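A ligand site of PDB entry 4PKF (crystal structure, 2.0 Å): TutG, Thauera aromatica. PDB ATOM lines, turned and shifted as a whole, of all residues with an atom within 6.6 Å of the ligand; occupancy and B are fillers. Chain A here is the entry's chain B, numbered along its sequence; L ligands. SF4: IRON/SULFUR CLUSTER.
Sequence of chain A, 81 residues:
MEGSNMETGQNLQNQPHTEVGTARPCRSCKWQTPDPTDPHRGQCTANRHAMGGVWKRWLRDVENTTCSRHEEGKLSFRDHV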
ATOM      1  N   ASN A  14      16.983  -0.366  21.212  1.00  0.00           N
ATOM      2  CA  ASN A  14      17.106   1.058  20.898  1.00  0.00           C
ATOM      3  C   ASN A  14      15.892   1.527  20.087  1.00  0.00           C
ATOM      4  O   ASN A  14      15.905   2.601  19.499  1.00  0.00           O
ATOM      5  CB  ASN A  14      18.415   1.337  20.136  1.00  0.00           C
ATOM      6  CG  ASN A  14      18.776   0.221  19.132  1.00  0.00           C
ATOM      7  OD1 ASN A  14      17.898  -0.399  18.523  1.00  0.00           O
ATOM      8  ND2 ASN A  14      20.074  -0.026  18.982  1.00  0.00           N
ATOM      9  N   GLN A  15      14.854   0.698  20.052  1.00  0.00           N
ATOM     10  CA  GLN A  15      13.567   1.064  19.456  1.00  0.00           C
ATOM     11  C   GLN A  15      12.513   0.976  20.526  1.00  0.00           C
ATOM     12  O   GLN A  15      12.639   0.181  21.448  1.00  0.00           O
ATOM     13  CB  GLN A  15      13.201   0.158  18.282  1.00  0.00           C
ATOM     14  CG  GLN A  15      13.755   0.599  16.943  1.00  0.00           C
ATOM     15  CD  GLN A  15      13.340  -0.357  15.839  1.00  0.00           C
ATOM     16  OE1 GLN A  15      14.070  -1.300  15.516  1.00  0.00           O
ATOM     17  NE2 GLN A  15      12.159  -0.124  15.273  1.00  0.00           N
ATOM     18  N   PRO A  16      11.459   1.816  20.420  1.00  0.00           N
ATOM     19  CA  PRO A  16      10.434   1.854  21.463  1.00  0.00           C
ATOM     20  C   PRO A  16       9.846   0.471  21.749  1.00  0.00           C
ATOM     21  O   PRO A  16       9.503  -0.259  20.831  1.00  0.00           O
ATOM     22  CB  PRO A  16       9.351   2.801  20.903  1.00  0.00           C
ATOM     23  CG  PRO A  16       9.764   3.124  19.472  1.00  0.00           C
ATOM     24  CD  PRO A  16      11.244   2.847  19.381  1.00  0.00           C
ATOM     25  N   HIS A  17       9.752   0.134  23.040  1.00  0.00           N
ATOM     26  CA  HIS A  17       9.182  -1.125  23.452  1.00  0.00           C
ATOM     27  C   HIS A  17       8.457  -0.987  24.806  1.00  0.00           C
ATOM     28  O   HIS A  17       8.819  -0.165  25.646  1.00  0.00           O
ATOM     29  CB  HIS A  17      10.256  -2.200  23.531  1.00  0.00           C
ATOM     30  CG  HIS A  17      11.316  -1.928  24.558  1.00  0.00           C
ATOM     31  ND1 HIS A  17      11.129  -2.182  25.908  1.00  0.00           N
ATOM     32  CD2 HIS A  17      12.558  -1.414  24.441  1.00  0.00           C
ATOM     33  CE1 HIS A  17      12.214  -1.837  26.567  1.00  0.00           C
ATOM     34  NE2 HIS A  17      13.101  -1.368  25.703  1.00  0.00           N
ATOM     35  N   ARG A  24      11.666   5.106  33.167  1.00  0.00           N
ATOM     36  CA  ARG A  24      12.075   5.976  32.071  1.00  0.00           C
ATOM     37  C   ARG A  24      11.042   5.974  30.948  1.00  0.00           C
ATOM     38  O   ARG A  24      11.313   5.483  29.855  1.00  0.00           O
ATOM     39  CB  ARG A  24      13.450   5.536  31.552  1.00  0.00           C
ATOM     40  CG  ARG A  24      14.566   5.767  32.590  1.00  0.00           C
ATOM     41  CD  ARG A  24      15.841   4.969  32.306  1.00  0.00           C
ATOM     42  NE  ARG A  24      16.723   5.031  33.477  1.00  0.00           N
ATOM     43  CZ  ARG A  24      17.944   4.501  33.545  1.00  0.00           C
ATOM     44  NH1 ARG A  24      18.461   3.869  32.493  1.00  0.00           N
ATOM     45  NH2 ARG A  24      18.657   4.620  34.663  1.00  0.00           N
ATOM     46  N   PRO A  25       9.844   6.508  31.234  1.00  0.00           N
ATOM     47  CA  PRO A  25       8.799   6.574  30.216  1.00  0.00           C
ATOM     48  C   PRO A  25       9.136   7.578  29.120  1.00  0.00           C
ATOM     49  O   PRO A  25       9.786   8.585  29.414  1.00  0.00           O
ATOM     50  CB  PRO A  25       7.582   7.046  31.018  1.00  0.00           C
ATOM     51  CG  PRO A  25       8.182   7.969  32.042  1.00  0.00           C
ATOM     52  CD  PRO A  25       9.466   7.265  32.453  1.00  0.00           C
ATOM     53  N   CYS A  26       8.698   7.304  27.894  1.00  0.00           N
ATOM     54  CA  CYS A  26       8.752   8.296  26.818  1.00  0.00           C
ATOM     55  C   CYS A  26       8.263   9.673  27.251  1.00  0.00           C
ATOM     56  O   CYS A  26       8.821  10.712  26.833  1.00  0.00           O
ATOM     57  CB  CYS A  26       7.948   7.819  25.632  1.00  0.00           C
ATOM     58  SG  CYS A  26       8.667   6.270  24.968  1.00  0.00           S
ATOM     59  N   ARG A  27       7.244   9.712  28.100  1.00  0.00           N
ATOM     60  CA  ARG A  27       6.677  10.989  28.526  1.00  0.00           C
ATOM     61  C   ARG A  27       7.725  11.969  29.076  1.00  0.00           C
ATOM     62  O   ARG A  27       7.589  13.184  28.934  1.00  0.00           O
ATOM     63  CB  ARG A  27       5.596  10.782  29.590  1.00  0.00           C
ATOM     64  CG  ARG A  27       4.787  12.032  29.805  1.00  0.00           C
ATOM     65  CD  ARG A  27       3.574  11.777  30.639  1.00  0.00           C
ATOM     66  NE  ARG A  27       2.907  13.037  30.941  1.00  0.00           N
ATOM     67  CZ  ARG A  27       1.917  13.153  31.815  1.00  0.00           C
ATOM     68  NH1 ARG A  27       1.481  12.080  32.464  1.00  0.00           N
ATOM     69  NH2 ARG A  27       1.375  14.338  32.046  1.00  0.00           N
ATOM     70  N   CYS A  29      11.034  11.829  28.292  1.00  0.00           N
ATOM     71  CA  CYS A  29      12.206  11.805  27.408  1.00  0.00           C
ATOM     72  C   CYS A  29      12.261  13.074  26.546  1.00  0.00           C
ATOM     73  O   CYS A  29      11.222  13.505  26.021  1.00  0.00           O
ATOM     74  CB  CYS A  29      12.176  10.564  26.500  1.00  0.00           C
ATOM     75  SG  CYS A  29      13.583  10.354  25.351  1.00  0.00           S
ATOM     76  N   LYS A  30      13.464  13.642  26.391  1.00  0.00           N
ATOM     77  CA  LYS A  30      13.649  14.858  25.596  1.00  0.00           C
ATOM     78  C   LYS A  30      13.313  14.652  24.121  1.00  0.00           C
ATOM     79  O   LYS A  30      13.012  15.606  23.410  1.00  0.00           O
ATOM     80  CB  LYS A  30      15.080  15.402  25.730  1.00  0.00           C
ATOM     81  CG  LYS A  30      16.129  14.660  24.924  1.00  0.00           C
ATOM     82  CD  LYS A  30      17.476  15.389  25.001  1.00  0.00           C
ATOM     83  CE  LYS A  30      18.586  14.594  24.320  1.00  0.00           C
ATOM     84  NZ  LYS A  30      19.893  15.350  24.295  1.00  0.00           N
ATOM     85  N   TRP A  31      13.378  13.408  23.670  1.00  0.00           N
ATOM     86  CA  TRP A  31      13.130  13.122  22.266  1.00  0.00           C
ATOM     87  C   TRP A  31      11.632  13.047  21.943  1.00  0.00           C
ATOM     88  O   TRP A  31      11.264  13.148  20.771  1.00  0.00           O
ATOM     89  CB  TRP A  31      13.796  11.811  21.866  1.00  0.00           C
ATOM     90  CG  TRP A  31      15.289  11.889  21.967  1.00  0.00           C
ATOM     91  CD1 TRP A  31      16.107  11.127  22.772  1.00  0.00           C
ATOM     92  CD2 TRP A  31      16.151  12.787  21.238  1.00  0.00           C
ATOM     93  NE1 TRP A  31      17.424  11.523  22.590  1.00  0.00           N
ATOM     94  CE2 TRP A  31      17.476  12.518  21.653  1.00  0.00           C
ATOM     95  CE3 TRP A  31      15.926  13.775  20.275  1.00  0.00           C
ATOM     96  CZ2 TRP A  31      18.567  13.212  21.140  1.00  0.00           C
ATOM     97  CZ3 TRP A  31      17.009  14.463  19.776  1.00  0.00           C
ATOM     98  CH2 TRP A  31      18.323  14.166  20.193  1.00  0.00           C
ATOM     99  N   GLN A  32      10.808  12.871  22.988  1.00  0.00           N
ATOM    100  CA  GLN A  32       9.351  12.776  22.851  1.00  0.00           C
ATOM    101  C   GLN A  32       8.693  14.158  22.782  1.00  0.00           C
ATOM    102  O   GLN A  32       9.116  15.073  23.476  1.00  0.00           O
ATOM    103  CB  GLN A  32       8.728  12.004  24.031  1.00  0.00           C
ATOM    104  CG  GLN A  32       7.260  11.590  23.874  1.00  0.00           C
ATOM    105  CD  GLN A  32       6.225  12.639  24.367  1.00  0.00           C
ATOM    106  OE1 GLN A  32       5.041  12.495  24.095  1.00  0.00           O
ATOM    107  NE2 GLN A  32       6.671  13.656  25.100  1.00  0.00           N
ATOM    108  N   THR A  33       7.683  14.291  21.934  1.00  0.00           N
ATOM    109  CA  THR A  33       6.759  15.440  21.985  1.00  0.00           C
ATOM    110  C   THR A  33       5.344  14.834  21.811  1.00  0.00           C
ATOM    111  O   THR A  33       5.175  13.795  21.135  1.00  0.00           O
ATOM    112  CB  THR A  33       7.138  16.527  20.910  1.00  0.00           C
ATOM    113  OG1 THR A  33       6.353  17.703  21.113  1.00  0.00           O
ATOM    114  CG2 THR A  33       6.888  16.048  19.498  1.00  0.00           C
ATOM    115  N   GLN A  43       5.078  11.333  20.061  1.00  0.00           N
ATOM    116  CA  GLN A  43       5.943  11.300  18.895  1.00  0.00           C
ATOM    117  C   GLN A  43       7.396  11.182  19.365  1.00  0.00           C
ATOM    118  O   GLN A  43       7.887  12.080  20.044  1.00  0.00           O
ATOM    119  CB  GLN A  43       5.809  12.563  18.028  1.00  0.00           C
ATOM    120  CG  GLN A  43       4.356  12.924  17.632  1.00  0.00           C
ATOM    121  CD  GLN A  43       4.273  14.243  16.867  1.00  0.00           C
ATOM    122  OE1 GLN A  43       4.674  14.316  15.696  1.00  0.00           O
ATOM    123  NE2 GLN A  43       3.764  15.285  17.538  1.00  0.00           N
ATOM    124  N   CYS A  44       8.068  10.095  18.983  1.00  0.00           N
ATOM    125  CA  CYS A  44       9.496   9.937  19.280  1.00  0.00           C
ATOM    126  C   CYS A  44      10.292  10.553  18.147  1.00  0.00           C
ATOM    127  O   CYS A  44      10.133  10.172  16.983  1.00  0.00           O
ATOM    128  CB  CYS A  44       9.883   8.462  19.457  1.00  0.00           C
ATOM    129  SG  CYS A  44      11.712   8.210  19.526  1.00  0.00           S
ATOM    130  N   THR A  45      11.156  11.517  18.477  1.00  0.00           N
ATOM    131  CA  THR A  45      11.883  12.221  17.427  1.00  0.00           C
ATOM    132  C   THR A  45      13.358  11.805  17.438  1.00  0.00           C
ATOM    133  O   THR A  45      14.191  12.479  16.838  1.00  0.00           O
ATOM    134  CB  THR A  45      11.766  13.766  17.580  1.00  0.00           C
ATOM    135  OG1 THR A  45      12.443  14.173  18.777  1.00  0.00           O
ATOM    136  CG2 THR A  45      10.271  14.221  17.684  1.00  0.00           C
ATOM    137  N   ALA A  46      13.671  10.677  18.063  1.00  0.00           N
ATOM    138  CA  ALA A  46      15.078  10.317  18.283  1.00  0.00           C
ATOM    139  C   ALA A  46      15.833   9.970  16.985  1.00  0.00           C
ATOM    140  O   ALA A  46      17.037  10.211  16.880  1.00  0.00           O
ATOM    141  CB  ALA A  46      15.151   9.162  19.263  1.00  0.00           C
ATOM    142  N   LEU A  59       4.004   6.896  19.188  1.00  0.00           N
ATOM    143  CA  LEU A  59       3.986   6.211  20.478  1.00  0.00           C
ATOM    144  C   LEU A  59       2.539   6.043  20.975  1.00  0.00           C
ATOM    145  O   LEU A  59       1.878   7.055  21.285  1.00  0.00           O
ATOM    146  CB  LEU A  59       4.818   6.995  21.506  1.00  0.00           C
ATOM    147  CG  LEU A  59       6.287   7.329  21.157  1.00  0.00           C
ATOM    148  CD1 LEU A  59       6.864   8.262  22.200  1.00  0.00           C
ATOM    149  CD2 LEU A  59       7.125   6.024  21.046  1.00  0.00           C
ATOM    150  N   THR A  65       6.191   2.884  27.831  1.00  0.00           N
ATOM    151  CA  THR A  65       7.101   2.616  26.735  1.00  0.00           C
ATOM    152  C   THR A  65       8.434   3.299  27.060  1.00  0.00           C
ATOM    153  O   THR A  65       8.471   4.296  27.794  1.00  0.00           O
ATOM    154  CB  THR A  65       6.534   3.094  25.365  1.00  0.00           C
ATOM    155  OG1 THR A  65       5.185   2.626  25.215  1.00  0.00           O
ATOM    156  CG2 THR A  65       7.353   2.565  24.216  1.00  0.00           C
ATOM    157  N   THR A  66       9.516   2.752  26.518  1.00  0.00           N
ATOM    158  CA  THR A  66      10.865   3.259  26.744  1.00  0.00           C
ATOM    159  C   THR A  66      11.783   2.682  25.695  1.00  0.00           C
ATOM    160  O   THR A  66      11.404   1.770  24.964  1.00  0.00           O
ATOM    161  CB  THR A  66      11.410   2.856  28.126  1.00  0.00           C
ATOM    162  OG1 THR A  66      12.587   3.614  28.416  1.00  0.00           O
ATOM    163  CG2 THR A  66      11.747   1.355  28.171  1.00  0.00           C
ATOM    164  N   CYS A  67      13.006   3.197  25.617  1.00  0.00           N
ATOM    165  CA  CYS A  67      14.055   2.524  24.857  1.00  0.00           C
ATOM    166  C   CYS A  67      15.404   2.895  25.462  1.00  0.00           C
ATOM    167  O   CYS A  67      15.454   3.662  26.416  1.00  0.00           O
ATOM    168  CB  CYS A  67      14.004   2.886  23.376  1.00  0.00           C
ATOM    169  SG  CYS A  67      14.796   4.460  22.969  1.00  0.00           S
ATOM    170  N   SER A  68      16.496   2.396  24.897  1.00  0.00           N
ATOM    171  CA  SER A  68      17.801   2.643  25.491  1.00  0.00           C
ATOM    172  C   SER A  68      18.245   4.095  25.261  1.00  0.00           C
ATOM    173  O   SER A  68      19.087   4.601  25.985  1.00  0.00           O
ATOM    174  CB  SER A  68      18.836   1.672  24.916  1.00  0.00           C
ATOM    175  OG  SER A  68      18.948   1.820  23.514  1.00  0.00           O
ATOM    176  N   ARG A  69      17.676   4.770  24.274  1.00  0.00           N
ATOM    177  CA  ARG A  69      18.099   6.141  24.016  1.00  0.00           C
ATOM    178  C   ARG A  69      17.430   7.141  24.970  1.00  0.00           C
ATOM    179  O   ARG A  69      17.713   8.335  24.895  1.00  0.00           O
ATOM    180  CB  ARG A  69      17.803   6.521  22.563  1.00  0.00           C
ATOM    181  CG  ARG A  69      18.557   5.654  21.541  1.00  0.00           C
ATOM    182  CD  ARG A  69      17.878   5.650  20.181  1.00  0.00           C
ATOM    183  NE  ARG A  69      16.458   5.353  20.321  1.00  0.00           N
ATOM    184  CZ  ARG A  69      15.552   5.446  19.337  1.00  0.00           C
ATOM    185  NH1 ARG A  69      15.963   5.812  18.123  1.00  0.00           N
ATOM    186  NH2 ARG A  69      14.264   5.152  19.578  1.00  0.00           N
ATOM    187  N   HIS A  70      16.602   6.656  25.885  1.00  0.00           N
ATOM    188  CA  HIS A  70      15.891   7.529  26.806  1.00  0.00           C
ATOM    189  C   HIS A  70      16.845   8.482  27.497  1.00  0.00           C
ATOM    190  O   HIS A  70      17.869   8.078  28.017  1.00  0.00           O
ATOM    191  CB  HIS A  70      15.127   6.732  27.855  1.00  0.00           C
ATOM    192  CG  HIS A  70      14.326   7.597  28.787  1.00  0.00           C
ATOM    193  ND1 HIS A  70      14.897   8.296  29.823  1.00  0.00           N
ATOM    194  CD2 HIS A  70      13.005   7.874  28.819  1.00  0.00           C
ATOM    195  CE1 HIS A  70      13.948   8.964  30.460  1.00  0.00           C
ATOM    196  NE2 HIS A  70      12.800   8.734  29.872  1.00  0.00           N
ATOM    197  N   GLU A  71      16.504   9.771  27.455  1.00  0.00           N
ATOM    198  CA  GLU A  71      17.259  10.799  28.149  1.00  0.00           C
ATOM    199  C   GLU A  71      16.296  11.837  28.689  1.00  0.00           C
ATOM    200  O   GLU A  71      15.596  12.506  27.932  1.00  0.00           O
ATOM    201  CB  GLU A  71      18.281  11.446  27.210  1.00  0.00           C
ATOM    202  CG  GLU A  71      19.179  12.470  27.861  1.00  0.00           C
ATOM    203  CD  GLU A  71      20.207  13.026  26.885  1.00  0.00           C
ATOM    204  OE1 GLU A  71      20.522  14.236  26.992  1.00  0.00           O
ATOM    205  OE2 GLU A  71      20.693  12.261  26.010  1.00  0.00           O
HETATM  206 FE1  SF4 L   1      12.796   8.587  24.167  1.00  0.00          FE
HETATM  207 FE2  SF4 L   1      11.850   7.740  21.791  1.00  0.00          FE
HETATM  208 FE3  SF4 L   1      10.660   6.838  24.040  1.00  0.00          FE
HETATM  209 FE4  SF4 L   1      13.152   5.979  23.442  1.00  0.00          FE
HETATM  210  S1  SF4 L   1      11.203   5.585  22.290  1.00  0.00           S
HETATM  211  S2  SF4 L   1      12.462   6.701  25.458  1.00  0.00           S
HETATM  212  S3  SF4 L   1      14.032   7.841  22.460  1.00  0.00           S
HETATM  213  S4  SF4 L   1      10.734   9.007  23.264  1.00  0.00           S
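FE1 of the ligand is bound by SG of Cys 29 (2.3 Å).
The side-chain sulfur (SG) of Cys 26 is bound to an iron atom (FE3) of the ligand (2.3 Å).
The backbone NH (N) of Cys 67 sits close to a sulfur (S2) of the ligand.
The side-chain sulfur (SG) of Cys 67 is bound to an iron atom (FE4) of the ligand (2.3 Å).
An iron atom (FE2) of the ligand is bound by the side-chain sulfur (SG) of Cys 44 (2.3 Å).
SG of Cys 29 sits close to N of Trp 31.
SG of Cys 29 lies close to N of Glu 71 (3.6 Å).
N of Cys 26 sits at hydrogen-bond distance from O of Thr 65, 3.0 Å away.
SG of Cys 67 lies close to N of Arg 69.
SG of Cys 44 sits close to N of Ala 46.
NE2 of His 70 sits at hydrogen-bond distance from O of Pro 25, at 3.1 Å.
The backbone carbonyl oxygen (O) of Trp 31 sits at hydrogen-bond distance from the side-chain hydroxyl (OG1) of Thr 45 (2.5 Å).
The backbone carbonyl oxygen of Asn 14 sits close to the guanidinium group of Arg 69, 2.9 Å away.
CB of Pro 16 touches S1 of the ligand, 3.6 Å away.
Trp 31 touches the ligand (CD1 to S3, 3.9 Å).
Gln 32 touches the ligand (CB to S4, 3.7 Å).
Ala 46 touches the ligand (CB to S3, 3.6 Å).
Arg 69 touches the ligand.
His 70 touches the ligand.
Hydrophobic or aromatic side chains within 4 Å of the ligand: Pro 16, Trp 31, Ala 46 and His 70.
Ten residues have an atom within 4 Å of the ligand: Pro 16, Cys 26, Cys 29, Trp 31, Gln 32, Cys 44, Ala 46, Cys 67, Arg 69 and His 70.
The nearest printed residue that does not touch the ligand is Thr 66 (4.01 Å).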
